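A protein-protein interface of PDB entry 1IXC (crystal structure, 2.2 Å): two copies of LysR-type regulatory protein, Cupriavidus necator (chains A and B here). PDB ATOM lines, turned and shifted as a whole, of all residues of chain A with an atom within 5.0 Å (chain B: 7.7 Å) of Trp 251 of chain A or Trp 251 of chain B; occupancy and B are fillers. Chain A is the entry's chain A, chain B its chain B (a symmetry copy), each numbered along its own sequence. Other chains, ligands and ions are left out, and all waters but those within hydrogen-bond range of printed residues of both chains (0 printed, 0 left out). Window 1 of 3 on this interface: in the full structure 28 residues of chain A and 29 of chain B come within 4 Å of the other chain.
O of Arg 250 of chain B lies within hydrogen-bond range of N of Arg 250 of chain A, 3.1 Å away. The guanidinium group (NH2) of Arg 104 of chain B sits at hydrogen-bond distance from the side-chain sulfur (SD) of Met 234 of chain A (3.7 Å). The side-chain sulfur (SD) of Met 234 of chain B sits close to the backbone carbonyl oxygen (O) of Tyr 103 of chain A, 3.5 Å away. O of Tyr 103 of chain B sits close to SD of Met 234 of chain A, at 3.3 Å. OD2 of Asp 253 of chain A lies within salt-bridge range of NH2 of Arg 104 of chain B (2.7 Å).
Printed residues of chain B within 4 Å of Met 234 of chain A: Tyr 103 and Arg 104. Of the printed residues of chain B, Arg 250 of chain A touches Ile 249 and Arg 250. Trp 251 of chain A touches two residues of chain B. Of the printed residues of chain B, Asp 253 of chain A touches Arg 104 (2.7 Å). Ala 231 of chain B touches none of the printed residues of chain A. Of the printed residues of chain A, Arg 250 of chain B touches Ile 249 and Arg 250. Trp 251 of chain B touches just these residues of chain A: Ile 249 and Trp 251. The nearest residue of chain B that does not touch Trp 251 of chain A is Tyr 103 of chain B (4.4 Å).
Among the printed residues, pairs that only touch across the chains: Ile 249 of chain A with Ile 249 of chain B (3.2 Å), Pro 252 of chain A with Arg 104 of chain B (3.4 Å), Arg 250 of chain A with Ile 249 of chain B (3.5 Å), Ile 249 of chain A with Arg 250 of chain B (3.6 Å), Pro 252 of chain A with Ala 248 of chain B (3.6 Å), Pro 252 of chain A with Ile 249 of chain B (3.6 Å), Trp 251 of chain A with Ile 249 of chain B (3.6 Å), Ile 249 of chain A with Trp 251 of chain B (3.7 Å), Ile 249 of chain A with Pro 252 of chain B (3.8 Å) and Trp 251 of chain A with Trp 251 of chain B (3.9 Å).
The indole nitrogen (NE1) of Trp 251 of chain A lies close to the backbone carbonyl oxygen (O) of Ile 249 of chain A. The backbone carbonyl oxygen of Ile 249 of chain B sits close to the indole nitrogen of Trp 251 of chain B, at 3.4 Å. O of Val 246 of chain B lies within hydrogen-bond range of NE1 of Trp 251 of chain B (3.1 Å). The side-chain hydroxyl of Tyr 103 of chain B is in hydrogen-bond range of the side-chain hydroxyl of Thr 227 of chain B, at 3.4 Å. NE1 of Trp 251 of chain A lies within hydrogen-bond range of O of Val 246 of chain A (3.0 Å).
Ile 249 of chain A touches Arg 250 of chain B, and with the chains exchanged Arg 250 of chain A touches Ile 249 of chain B. Ile 249 of chain A touches Trp 251 of chain B, and with the chains exchanged Trp 251 of chain A touches Ile 249 of chain B. Ile 249 of chain A touches Pro 252 of chain B, and with the chains exchanged Pro 252 of chain A touches Ile 249 of chain B. Trp 251 of chain A touches its own counterpart, Trp 251 of chain B.
Hydrophobic or aromatic side chains of chain A that line the printed part of chain B: Met 234, Ile 249, Trp 251 and Pro 252. Printed residues of chain B that touch a printed residue of chain A: Tyr 103, Arg 104, Met 234, Ala 248, Ile 249, Arg 250, Trp 251 and Pro 252. Hydrophobic or aromatic side chains of chain B that line the printed part of chain A: Met 234, Ile 249, Trp 251 and Pro 252. Among the printed residues, Asp or Glu carboxylates within 4 Å of a Lys or Arg side-chain nitrogen of the other chain: Asp 253 of chain A with Arg 104 of chain B (2.7 Å).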
ATOM      1  N   TYR A 103      18.909 -10.604  16.640  1.00  0.00           N
ATOM      2  CA  TYR A 103      19.904  -9.715  16.020  1.00  0.00           C
ATOM      3  C   TYR A 103      20.190  -8.415  16.761  1.00  0.00           C
ATOM      4  O   TYR A 103      21.305  -7.903  16.699  1.00  0.00           O
ATOM      5  CB  TYR A 103      19.492  -9.398  14.585  1.00  0.00           C
ATOM      6  CG  TYR A 103      19.708 -10.573  13.682  1.00  0.00           C
ATOM      7  CD1 TYR A 103      18.700 -11.484  13.447  1.00  0.00           C
ATOM      8  CD2 TYR A 103      20.948 -10.810  13.111  1.00  0.00           C
ATOM      9  CE1 TYR A 103      18.906 -12.575  12.642  1.00  0.00           C
ATOM     10  CE2 TYR A 103      21.162 -11.910  12.309  1.00  0.00           C
ATOM     11  CZ  TYR A 103      20.138 -12.788  12.084  1.00  0.00           C
ATOM     12  OH  TYR A 103      20.338 -13.866  11.281  1.00  0.00           O
ATOM     13  N   LEU A 230      19.601 -13.332   3.831  1.00  0.00           N
ATOM     14  CA  LEU A 230      20.719 -12.392   3.838  1.00  0.00           C
ATOM     15  C   LEU A 230      21.922 -12.876   3.024  1.00  0.00           C
ATOM     16  O   LEU A 230      22.523 -12.106   2.272  1.00  0.00           O
ATOM     17  CB  LEU A 230      21.146 -12.112   5.278  1.00  0.00           C
ATOM     18  CG  LEU A 230      20.176 -11.259   6.099  1.00  0.00           C
ATOM     19  CD1 LEU A 230      20.478 -11.360   7.596  1.00  0.00           C
ATOM     20  CD2 LEU A 230      20.206  -9.807   5.632  1.00  0.00           C
ATOM     21  N   MET A 234      23.345 -11.011  -0.026  1.00  0.00           N
ATOM     22  CA  MET A 234      24.740 -10.648  -0.115  1.00  0.00           C
ATOM     23  C   MET A 234      25.401 -11.244  -1.351  1.00  0.00           C
ATOM     24  O   MET A 234      26.271 -10.627  -1.944  1.00  0.00           O
ATOM     25  CB  MET A 234      25.452 -11.145   1.133  1.00  0.00           C
ATOM     26  CG  MET A 234      26.955 -10.898   1.136  1.00  0.00           C
ATOM     27  SD  MET A 234      27.797 -11.538   2.777  1.00  0.00           S
ATOM     28  CE  MET A 234      26.512 -10.809   4.101  1.00  0.00           C
ATOM     29  N   VAL A 246      17.674  -6.486  12.083  1.00  0.00           N
ATOM     30  CA  VAL A 246      18.603  -6.928  11.058  1.00  0.00           C
ATOM     31  C   VAL A 246      19.300  -5.720  10.397  1.00  0.00           C
ATOM     32  O   VAL A 246      20.505  -5.752  10.139  1.00  0.00           O
ATOM     33  CB  VAL A 246      17.879  -7.835  10.002  1.00  0.00           C
ATOM     34  CG1 VAL A 246      18.790  -8.195   8.856  1.00  0.00           C
ATOM     35  CG2 VAL A 246      17.326  -9.122  10.655  1.00  0.00           C
ATOM     36  N   ILE A 249      22.482  -3.724  11.599  1.00  0.00           N
ATOM     37  CA  ILE A 249      23.783  -4.336  11.365  1.00  0.00           C
ATOM     38  C   ILE A 249      24.233  -3.957   9.960  1.00  0.00           C
ATOM     39  O   ILE A 249      23.450  -3.969   9.008  1.00  0.00           O
ATOM     40  CB  ILE A 249      23.663  -5.877  11.551  1.00  0.00           C
ATOM     41  CG1 ILE A 249      23.308  -6.185  13.011  1.00  0.00           C
ATOM     42  CG2 ILE A 249      24.951  -6.611  11.170  1.00  0.00           C
ATOM     43  CD1 ILE A 249      22.639  -7.549  13.213  1.00  0.00           C
ATOM     44  N   ARG A 250      25.494  -3.579   9.833  1.00  0.00           N
ATOM     45  CA  ARG A 250      26.038  -3.257   8.529  1.00  0.00           C
ATOM     46  C   ARG A 250      26.666  -4.509   7.889  1.00  0.00           C
ATOM     47  O   ARG A 250      27.713  -5.000   8.319  1.00  0.00           O
ATOM     48  CB  ARG A 250      27.028  -2.133   8.666  1.00  0.00           C
ATOM     49  CG  ARG A 250      27.400  -1.533   7.346  1.00  0.00           C
ATOM     50  CD  ARG A 250      28.092  -0.201   7.468  1.00  0.00           C
ATOM     51  NE  ARG A 250      28.730   0.115   6.205  1.00  0.00           N
ATOM     52  CZ  ARG A 250      30.034   0.040   5.972  1.00  0.00           C
ATOM     53  NH1 ARG A 250      30.886  -0.314   6.932  1.00  0.00           N
ATOM     54  NH2 ARG A 250      30.490   0.346   4.762  1.00  0.00           N
ATOM     55  N   TRP A 251      25.975  -5.055   6.901  1.00  0.00           N
ATOM     56  CA  TRP A 251      26.425  -6.258   6.221  1.00  0.00           C
ATOM     57  C   TRP A 251      27.094  -5.880   4.900  1.00  0.00           C
ATOM     58  O   TRP A 251      26.549  -5.128   4.112  1.00  0.00           O
ATOM     59  CB  TRP A 251      25.253  -7.199   5.917  1.00  0.00           C
ATOM     60  CG  TRP A 251      24.303  -7.449   7.042  1.00  0.00           C
ATOM     61  CD1 TRP A 251      23.274  -6.643   7.452  1.00  0.00           C
ATOM     62  CD2 TRP A 251      24.255  -8.607   7.873  1.00  0.00           C
ATOM     63  NE1 TRP A 251      22.610  -7.229   8.506  1.00  0.00           N
ATOM     64  CE2 TRP A 251      23.188  -8.440   8.773  1.00  0.00           C
ATOM     65  CE3 TRP A 251      25.013  -9.775   7.948  1.00  0.00           C
ATOM     66  CZ2 TRP A 251      22.870  -9.381   9.737  1.00  0.00           C
ATOM     67  CZ3 TRP A 251      24.695 -10.715   8.923  1.00  0.00           C
ATOM     68  CH2 TRP A 251      23.629 -10.517   9.796  1.00  0.00           C
ATOM     69  N   PRO A 252      28.284  -6.388   4.657  1.00  0.00           N
ATOM     70  CA  PRO A 252      28.959  -6.118   3.385  1.00  0.00           C
ATOM     71  C   PRO A 252      28.077  -6.514   2.187  1.00  0.00           C
ATOM     72  O   PRO A 252      27.460  -7.589   2.196  1.00  0.00           O
ATOM     73  CB  PRO A 252      30.212  -7.001   3.445  1.00  0.00           C
ATOM     74  CG  PRO A 252      30.391  -7.370   4.872  1.00  0.00           C
ATOM     75  CD  PRO A 252      29.072  -7.243   5.558  1.00  0.00           C
ATOM     76  N   ASP A 253      28.012  -5.634   1.187  1.00  0.00           N
ATOM     77  CA  ASP A 253      27.228  -5.840  -0.029  1.00  0.00           C
ATOM     78  C   ASP A 253      25.709  -5.833   0.144  1.00  0.00           C
ATOM     79  O   ASP A 253      24.990  -6.157  -0.799  1.00  0.00           O
ATOM     80  CB  ASP A 253      27.668  -7.111  -0.763  1.00  0.00           C
ATOM     81  CG  ASP A 253      29.147  -7.103  -1.093  1.00  0.00           C
ATOM     82  OD1 ASP A 253      29.669  -6.014  -1.431  1.00  0.00           O
ATOM     83  OD2 ASP A 253      29.863  -8.126  -1.025  1.00  0.00           O
ATOM     84  N   ILE A 254      25.203  -5.466   1.315  1.00  0.00           N
ATOM     85  CA  ILE A 254      23.761  -5.312   1.460  1.00  0.00           C
ATOM     86  C   ILE A 254      23.409  -3.855   1.753  1.00  0.00           C
ATOM     87  O   ILE A 254      24.054  -3.217   2.566  1.00  0.00           O
ATOM     88  CB  ILE A 254      23.185  -6.243   2.560  1.00  0.00           C
ATOM     89  CG1 ILE A 254      23.583  -7.695   2.272  1.00  0.00           C
ATOM     90  CG2 ILE A 254      21.687  -6.075   2.645  1.00  0.00           C
ATOM     91  CD1 ILE A 254      22.975  -8.719   3.209  1.00  0.00           C
ATOM     92  N   PHE A 256      20.008  -1.170   2.619  1.00  0.00           N
ATOM     93  CA  PHE A 256      18.701  -1.186   3.231  1.00  0.00           C
ATOM     94  C   PHE A 256      17.926   0.078   2.882  1.00  0.00           C
ATOM     95  O   PHE A 256      18.507   1.133   2.689  1.00  0.00           O
ATOM     96  CB  PHE A 256      18.837  -1.282   4.761  1.00  0.00           C
ATOM     97  CG  PHE A 256      19.387  -2.599   5.251  1.00  0.00           C
ATOM     98  CD1 PHE A 256      20.569  -2.651   5.977  1.00  0.00           C
ATOM     99  CD2 PHE A 256      18.721  -3.779   4.993  1.00  0.00           C
ATOM    100  CE1 PHE A 256      21.067  -3.863   6.428  1.00  0.00           C
ATOM    101  CE2 PHE A 256      19.208  -4.975   5.441  1.00  0.00           C
ATOM    102  CZ  PHE A 256      20.389  -5.014   6.154  1.00  0.00           C
ATOM    103  N   ILE B 102      28.932 -19.004   6.298  1.00  0.00           N
ATOM    104  CA  ILE B 102      27.726 -18.437   5.758  1.00  0.00           C
ATOM    105  C   ILE B 102      27.713 -16.901   5.862  1.00  0.00           C
ATOM    106  O   ILE B 102      27.006 -16.253   5.111  1.00  0.00           O
ATOM    107  CB  ILE B 102      26.500 -19.067   6.448  1.00  0.00           C
ATOM    108  CG1 ILE B 102      25.208 -18.686   5.734  1.00  0.00           C
ATOM    109  CG2 ILE B 102      26.416 -18.656   7.922  1.00  0.00           C
ATOM    110  CD1 ILE B 102      25.127 -19.197   4.311  1.00  0.00           C
ATOM    111  N   TYR B 103      28.537 -16.334   6.753  1.00  0.00           N
ATOM    112  CA  TYR B 103      28.533 -14.879   7.004  1.00  0.00           C
ATOM    113  C   TYR B 103      29.184 -14.066   5.908  1.00  0.00           C
ATOM    114  O   TYR B 103      28.744 -12.943   5.642  1.00  0.00           O
ATOM    115  CB  TYR B 103      29.193 -14.526   8.350  1.00  0.00           C
ATOM    116  CG  TYR B 103      28.353 -14.900   9.544  1.00  0.00           C
ATOM    117  CD1 TYR B 103      28.572 -16.081  10.214  1.00  0.00           C
ATOM    118  CD2 TYR B 103      27.311 -14.087   9.981  1.00  0.00           C
ATOM    119  CE1 TYR B 103      27.810 -16.438  11.297  1.00  0.00           C
ATOM    120  CE2 TYR B 103      26.525 -14.447  11.073  1.00  0.00           C
ATOM    121  CZ  TYR B 103      26.795 -15.631  11.724  1.00  0.00           C
ATOM    122  OH  TYR B 103      26.065 -16.050  12.810  1.00  0.00           O
ATOM    123  N   ARG B 104      30.209 -14.612   5.253  1.00  0.00           N
ATOM    124  CA  ARG B 104      30.882 -13.864   4.196  1.00  0.00           C
ATOM    125  C   ARG B 104      31.491 -14.711   3.068  1.00  0.00           C
ATOM    126  O   ARG B 104      31.170 -14.520   1.889  1.00  0.00           O
ATOM    127  CB  ARG B 104      31.979 -13.009   4.829  1.00  0.00           C
ATOM    128  CG  ARG B 104      32.583 -11.946   3.916  1.00  0.00           C
ATOM    129  CD  ARG B 104      31.576 -10.969   3.324  1.00  0.00           C
ATOM    130  NE  ARG B 104      32.260  -9.979   2.495  1.00  0.00           N
ATOM    131  CZ  ARG B 104      31.728  -9.366   1.464  1.00  0.00           C
ATOM    132  NH1 ARG B 104      32.454  -8.495   0.787  1.00  0.00           N
ATOM    133  NH2 ARG B 104      30.465  -9.612   1.105  1.00  0.00           N
ATOM    134  N   ALA B 168      36.288 -10.762  20.075  1.00  0.00           N
ATOM    135  CA  ALA B 168      35.088  -9.958  20.072  1.00  0.00           C
ATOM    136  C   ALA B 168      34.731  -9.580  21.523  1.00  0.00           C
ATOM    137  O   ALA B 168      34.695 -10.437  22.403  1.00  0.00           O
ATOM    138  CB  ALA B 168      33.938 -10.724  19.398  1.00  0.00           C
ATOM    139  N   VAL B 169      34.450  -8.302  21.761  1.00  0.00           N
ATOM    140  CA  VAL B 169      34.094  -7.824  23.096  1.00  0.00           C
ATOM    141  C   VAL B 169      33.032  -6.740  22.995  1.00  0.00           C
ATOM    142  O   VAL B 169      32.863  -6.129  21.946  1.00  0.00           O
ATOM    143  CB  VAL B 169      35.321  -7.236  23.833  1.00  0.00           C
ATOM    144  CG1 VAL B 169      36.326  -8.311  24.154  1.00  0.00           C
ATOM    145  CG2 VAL B 169      35.997  -6.145  23.003  1.00  0.00           C
ATOM    146  N   ARG B 171      31.358  -3.158  23.281  1.00  0.00           N
ATOM    147  CA  ARG B 171      31.895  -1.844  22.933  1.00  0.00           C
ATOM    148  C   ARG B 171      32.677  -1.179  24.077  1.00  0.00           C
ATOM    149  O   ARG B 171      33.698  -0.528  23.851  1.00  0.00           O
ATOM    150  CB  ARG B 171      30.720  -0.960  22.449  1.00  0.00           C
ATOM    151  CG  ARG B 171      30.549   0.423  23.074  1.00  0.00           C
ATOM    152  CD  ARG B 171      29.080   0.766  23.439  1.00  0.00           C
ATOM    153  NE  ARG B 171      28.903   0.940  24.887  1.00  0.00           N
ATOM    154  CZ  ARG B 171      27.752   1.229  25.492  1.00  0.00           C
ATOM    155  NH1 ARG B 171      26.626   1.366  24.791  1.00  0.00           N
ATOM    156  NH2 ARG B 171      27.726   1.380  26.813  1.00  0.00           N
ATOM    157  N   ALA B 226      27.536 -19.313  16.763  1.00  0.00           N
ATOM    158  CA  ALA B 226      28.084 -17.963  16.715  1.00  0.00           C
ATOM    159  C   ALA B 226      27.044 -16.898  17.065  1.00  0.00           C
ATOM    160  O   ALA B 226      27.355 -15.904  17.714  1.00  0.00           O
ATOM    161  CB  ALA B 226      28.651 -17.700  15.338  1.00  0.00           C
ATOM    162  N   THR B 227      25.813 -17.116  16.623  1.00  0.00           N
ATOM    163  CA  THR B 227      24.690 -16.236  16.934  1.00  0.00           C
ATOM    164  C   THR B 227      24.565 -16.051  18.449  1.00  0.00           C
ATOM    165  O   THR B 227      24.440 -14.942  18.924  1.00  0.00           O
ATOM    166  CB  THR B 227      23.419 -16.843  16.338  1.00  0.00           C
ATOM    167  OG1 THR B 227      23.483 -16.751  14.913  1.00  0.00           O
ATOM    168  CG2 THR B 227      22.186 -16.076  16.695  1.00  0.00           C
ATOM    169  N   LEU B 230      27.562 -14.023  19.729  1.00  0.00           N
ATOM    170  CA  LEU B 230      27.513 -12.629  19.291  1.00  0.00           C
ATOM    171  C   LEU B 230      26.449 -11.895  20.085  1.00  0.00           C
ATOM    172  O   LEU B 230      26.652 -10.753  20.518  1.00  0.00           O
ATOM    173  CB  LEU B 230      27.248 -12.501  17.775  1.00  0.00           C
ATOM    174  CG  LEU B 230      28.412 -12.925  16.855  1.00  0.00           C
ATOM    175  CD1 LEU B 230      27.935 -13.327  15.458  1.00  0.00           C
ATOM    176  CD2 LEU B 230      29.484 -11.843  16.784  1.00  0.00           C
ATOM    177  N   ALA B 231      25.320 -12.560  20.298  1.00  0.00           N
ATOM    178  CA  ALA B 231      24.234 -11.952  21.052  1.00  0.00           C
ATOM    179  C   ALA B 231      24.623 -11.745  22.524  1.00  0.00           C
ATOM    180  O   ALA B 231      24.290 -10.723  23.112  1.00  0.00           O
ATOM    181  CB  ALA B 231      23.006 -12.782  20.925  1.00  0.00           C
ATOM    182  N   MET B 234      27.059  -8.703  22.433  1.00  0.00           N
ATOM    183  CA  MET B 234      26.266  -7.509  22.248  1.00  0.00           C
ATOM    184  C   MET B 234      25.549  -7.106  23.528  1.00  0.00           C
ATOM    185  O   MET B 234      25.405  -5.934  23.810  1.00  0.00           O
ATOM    186  CB  MET B 234      25.241  -7.724  21.131  1.00  0.00           C
ATOM    187  CG  MET B 234      24.581  -6.476  20.698  1.00  0.00           C
ATOM    188  SD  MET B 234      23.293  -6.768  19.286  1.00  0.00           S
ATOM    189  CE  MET B 234      24.482  -7.148  17.804  1.00  0.00           C
ATOM    190  N   VAL B 242      36.078 -15.212  17.060  1.00  0.00           N
ATOM    191  CA  VAL B 242      35.325 -15.469  15.834  1.00  0.00           C
ATOM    192  C   VAL B 242      36.211 -15.291  14.616  1.00  0.00           C
ATOM    193  O   VAL B 242      37.123 -14.459  14.633  1.00  0.00           O
ATOM    194  CB  VAL B 242      34.170 -14.474  15.683  1.00  0.00           C
ATOM    195  CG1 VAL B 242      33.308 -14.460  16.936  1.00  0.00           C
ATOM    196  CG2 VAL B 242      34.695 -13.073  15.400  1.00  0.00           C
ATOM    197  N   SER B 245      35.110 -13.771   8.848  1.00  0.00           N
ATOM    198  CA  SER B 245      33.808 -13.637   8.194  1.00  0.00           C
ATOM    199  C   SER B 245      32.862 -12.834   9.098  1.00  0.00           C
ATOM    200  O   SER B 245      32.165 -11.938   8.654  1.00  0.00           O
ATOM    201  CB  SER B 245      33.189 -15.018   7.934  1.00  0.00           C
ATOM    202  OG  SER B 245      33.470 -15.501   6.615  1.00  0.00           O
ATOM    203  N   VAL B 246      32.860 -13.190  10.370  1.00  0.00           N
ATOM    204  CA  VAL B 246      32.036 -12.539  11.365  1.00  0.00           C
ATOM    205  C   VAL B 246      32.512 -11.104  11.616  1.00  0.00           C
ATOM    206  O   VAL B 246      31.695 -10.185  11.651  1.00  0.00           O
ATOM    207  CB  VAL B 246      32.002 -13.369  12.655  1.00  0.00           C
ATOM    208  CG1 VAL B 246      31.115 -12.700  13.727  1.00  0.00           C
ATOM    209  CG2 VAL B 246      31.495 -14.777  12.339  1.00  0.00           C
ATOM    210  N   ALA B 247      33.828 -10.902  11.707  1.00  0.00           N
ATOM    211  CA  ALA B 247      34.385  -9.581  12.009  1.00  0.00           C
ATOM    212  C   ALA B 247      34.235  -8.590  10.862  1.00  0.00           C
ATOM    213  O   ALA B 247      34.394  -7.397  11.067  1.00  0.00           O
ATOM    214  CB  ALA B 247      35.855  -9.690  12.417  1.00  0.00           C
ATOM    215  N   ALA B 248      33.943  -9.087   9.663  1.00  0.00           N
ATOM    216  CA  ALA B 248      33.706  -8.226   8.500  1.00  0.00           C
ATOM    217  C   ALA B 248      32.368  -7.459   8.595  1.00  0.00           C
ATOM    218  O   ALA B 248      32.154  -6.486   7.898  1.00  0.00           O
ATOM    219  CB  ALA B 248      33.743  -9.057   7.204  1.00  0.00           C
ATOM    220  N   ILE B 249      31.471  -7.915   9.456  1.00  0.00           N
ATOM    221  CA  ILE B 249      30.166  -7.295   9.641  1.00  0.00           C
ATOM    222  C   ILE B 249      30.255  -6.345  10.844  1.00  0.00           C
ATOM    223  O   ILE B 249      30.896  -6.675  11.828  1.00  0.00           O
ATOM    224  CB  ILE B 249      29.153  -8.428   9.871  1.00  0.00           C
ATOM    225  CG1 ILE B 249      29.002  -9.243   8.585  1.00  0.00           C
ATOM    226  CG2 ILE B 249      27.796  -7.917  10.325  1.00  0.00           C
ATOM    227  CD1 ILE B 249      28.437 -10.630   8.823  1.00  0.00           C
ATOM    228  N   ARG B 250      29.671  -5.152  10.737  1.00  0.00           N
ATOM    229  CA  ARG B 250      29.602  -4.213  11.868  1.00  0.00           C
ATOM    230  C   ARG B 250      28.342  -4.467  12.706  1.00  0.00           C
ATOM    231  O   ARG B 250      27.246  -4.101  12.320  1.00  0.00           O
ATOM    232  CB  ARG B 250      29.616  -2.751  11.384  1.00  0.00           C
ATOM    233  CG  ARG B 250      29.875  -1.709  12.506  1.00  0.00           C
ATOM    234  CD  ARG B 250      29.508  -0.236  12.162  1.00  0.00           C
ATOM    235  NE  ARG B 250      29.988   0.664  13.219  1.00  0.00           N
ATOM    236  CZ  ARG B 250      29.348   0.913  14.360  1.00  0.00           C
ATOM    237  NH1 ARG B 250      28.153   0.366  14.620  1.00  0.00           N
ATOM    238  NH2 ARG B 250      29.908   1.720  15.253  1.00  0.00           N
ATOM    239  N   TRP B 251      28.523  -5.099  13.864  1.00  0.00           N
ATOM    240  CA  TRP B 251      27.426  -5.396  14.791  1.00  0.00           C
ATOM    241  C   TRP B 251      27.436  -4.314  15.850  1.00  0.00           C
ATOM    242  O   TRP B 251      28.488  -4.059  16.445  1.00  0.00           O
ATOM    243  CB  TRP B 251      27.645  -6.731  15.479  1.00  0.00           C
ATOM    244  CG  TRP B 251      28.077  -7.848  14.592  1.00  0.00           C
ATOM    245  CD1 TRP B 251      29.344  -8.132  14.189  1.00  0.00           C
ATOM    246  CD2 TRP B 251      27.245  -8.880  14.057  1.00  0.00           C
ATOM    247  NE1 TRP B 251      29.349  -9.252  13.391  1.00  0.00           N
ATOM    248  CE2 TRP B 251      28.070  -9.733  13.296  1.00  0.00           C
ATOM    249  CE3 TRP B 251      25.873  -9.144  14.100  1.00  0.00           C
ATOM    250  CZ2 TRP B 251      27.573 -10.834  12.602  1.00  0.00           C
ATOM    251  CZ3 TRP B 251      25.383 -10.255  13.413  1.00  0.00           C
ATOM    252  CH2 TRP B 251      26.232 -11.079  12.678  1.00  0.00           C
ATOM    253  N   PRO B 252      26.300  -3.670  16.114  1.00  0.00           N
ATOM    254  CA  PRO B 252      26.311  -2.578  17.077  1.00  0.00           C
ATOM    255  C   PRO B 252      26.733  -3.124  18.428  1.00  0.00           C
ATOM    256  O   PRO B 252      26.339  -4.250  18.803  1.00  0.00           O
ATOM    257  CB  PRO B 252      24.855  -2.096  17.099  1.00  0.00           C
ATOM    258  CG  PRO B 252      24.247  -2.610  15.884  1.00  0.00           C
ATOM    259  CD  PRO B 252      24.947  -3.913  15.597  1.00  0.00           C
ATOM    260  N   ASP B 253      27.551  -2.345  19.120  1.00  0.00           N
ATOM    261  CA  ASP B 253      28.044  -2.655  20.455  1.00  0.00           C
ATOM    262  C   ASP B 253      29.095  -3.750  20.546  1.00  0.00           C
ATOM    263  O   ASP B 253      29.563  -4.046  21.638  1.00  0.00           O
ATOM    264  CB  ASP B 253      26.899  -2.938  21.422  1.00  0.00           C
ATOM    265  CG  ASP B 253      25.957  -1.772  21.543  1.00  0.00           C
ATOM    266  OD1 ASP B 253      26.402  -0.622  21.351  1.00  0.00           O
ATOM    267  OD2 ASP B 253      24.754  -1.909  21.811  1.00  0.00           O
ATOM    268  N   ILE B 254      29.506  -4.325  19.428  1.00  0.00           N
ATOM    269  CA  ILE B 254      30.614  -5.265  19.459  1.00  0.00           C
ATOM    270  C   ILE B 254      31.816  -4.645  18.761  1.00  0.00           C
ATOM    271  O   ILE B 254      31.664  -4.018  17.720  1.00  0.00           O
ATOM    272  CB  ILE B 254      30.227  -6.606  18.800  1.00  0.00           C
ATOM    273  CG1 ILE B 254      29.035  -7.228  19.530  1.00  0.00           C
ATOM    274  CG2 ILE B 254      31.425  -7.581  18.807  1.00  0.00           C
ATOM    275  CD1 ILE B 254      28.303  -8.250  18.735  1.00  0.00           C
ATOM    276  N   ALA B 255      32.989  -4.776  19.385  1.00  0.00           N
ATOM    277  CA  ALA B 255      34.266  -4.360  18.817  1.00  0.00           C
ATOM    278  C   ALA B 255      35.141  -5.598  18.605  1.00  0.00           C
ATOM    279  O   ALA B 255      35.054  -6.561  19.356  1.00  0.00           O
ATOM    280  CB  ALA B 255      34.981  -3.376  19.740  1.00  0.00           C
ATOM    281  N   PHE B 256      35.996  -5.552  17.590  1.00  0.00           N
ATOM    282  CA  PHE B 256      36.863  -6.670  17.264  1.00  0.00           C
ATOM    283  C   PHE B 256      38.339  -6.270  17.312  1.00  0.00           C
ATOM    284  O   PHE B 256      38.703  -5.103  17.120  1.00  0.00           O
ATOM    285  CB  PHE B 256      36.530  -7.224  15.864  1.00  0.00           C
ATOM    286  CG  PHE B 256      35.138  -7.760  15.735  1.00  0.00           C
ATOM    287  CD1 PHE B 256      34.142  -6.995  15.164  1.00  0.00           C
ATOM    288  CD2 PHE B 256      34.824  -9.035  16.176  1.00  0.00           C
ATOM    289  CE1 PHE B 256      32.861  -7.480  15.036  1.00  0.00           C
ATOM    290  CE2 PHE B 256      33.527  -9.523  16.060  1.00  0.00           C
ATOM    291  CZ  PHE B 256      32.556  -8.747  15.481  1.00  0.00           C
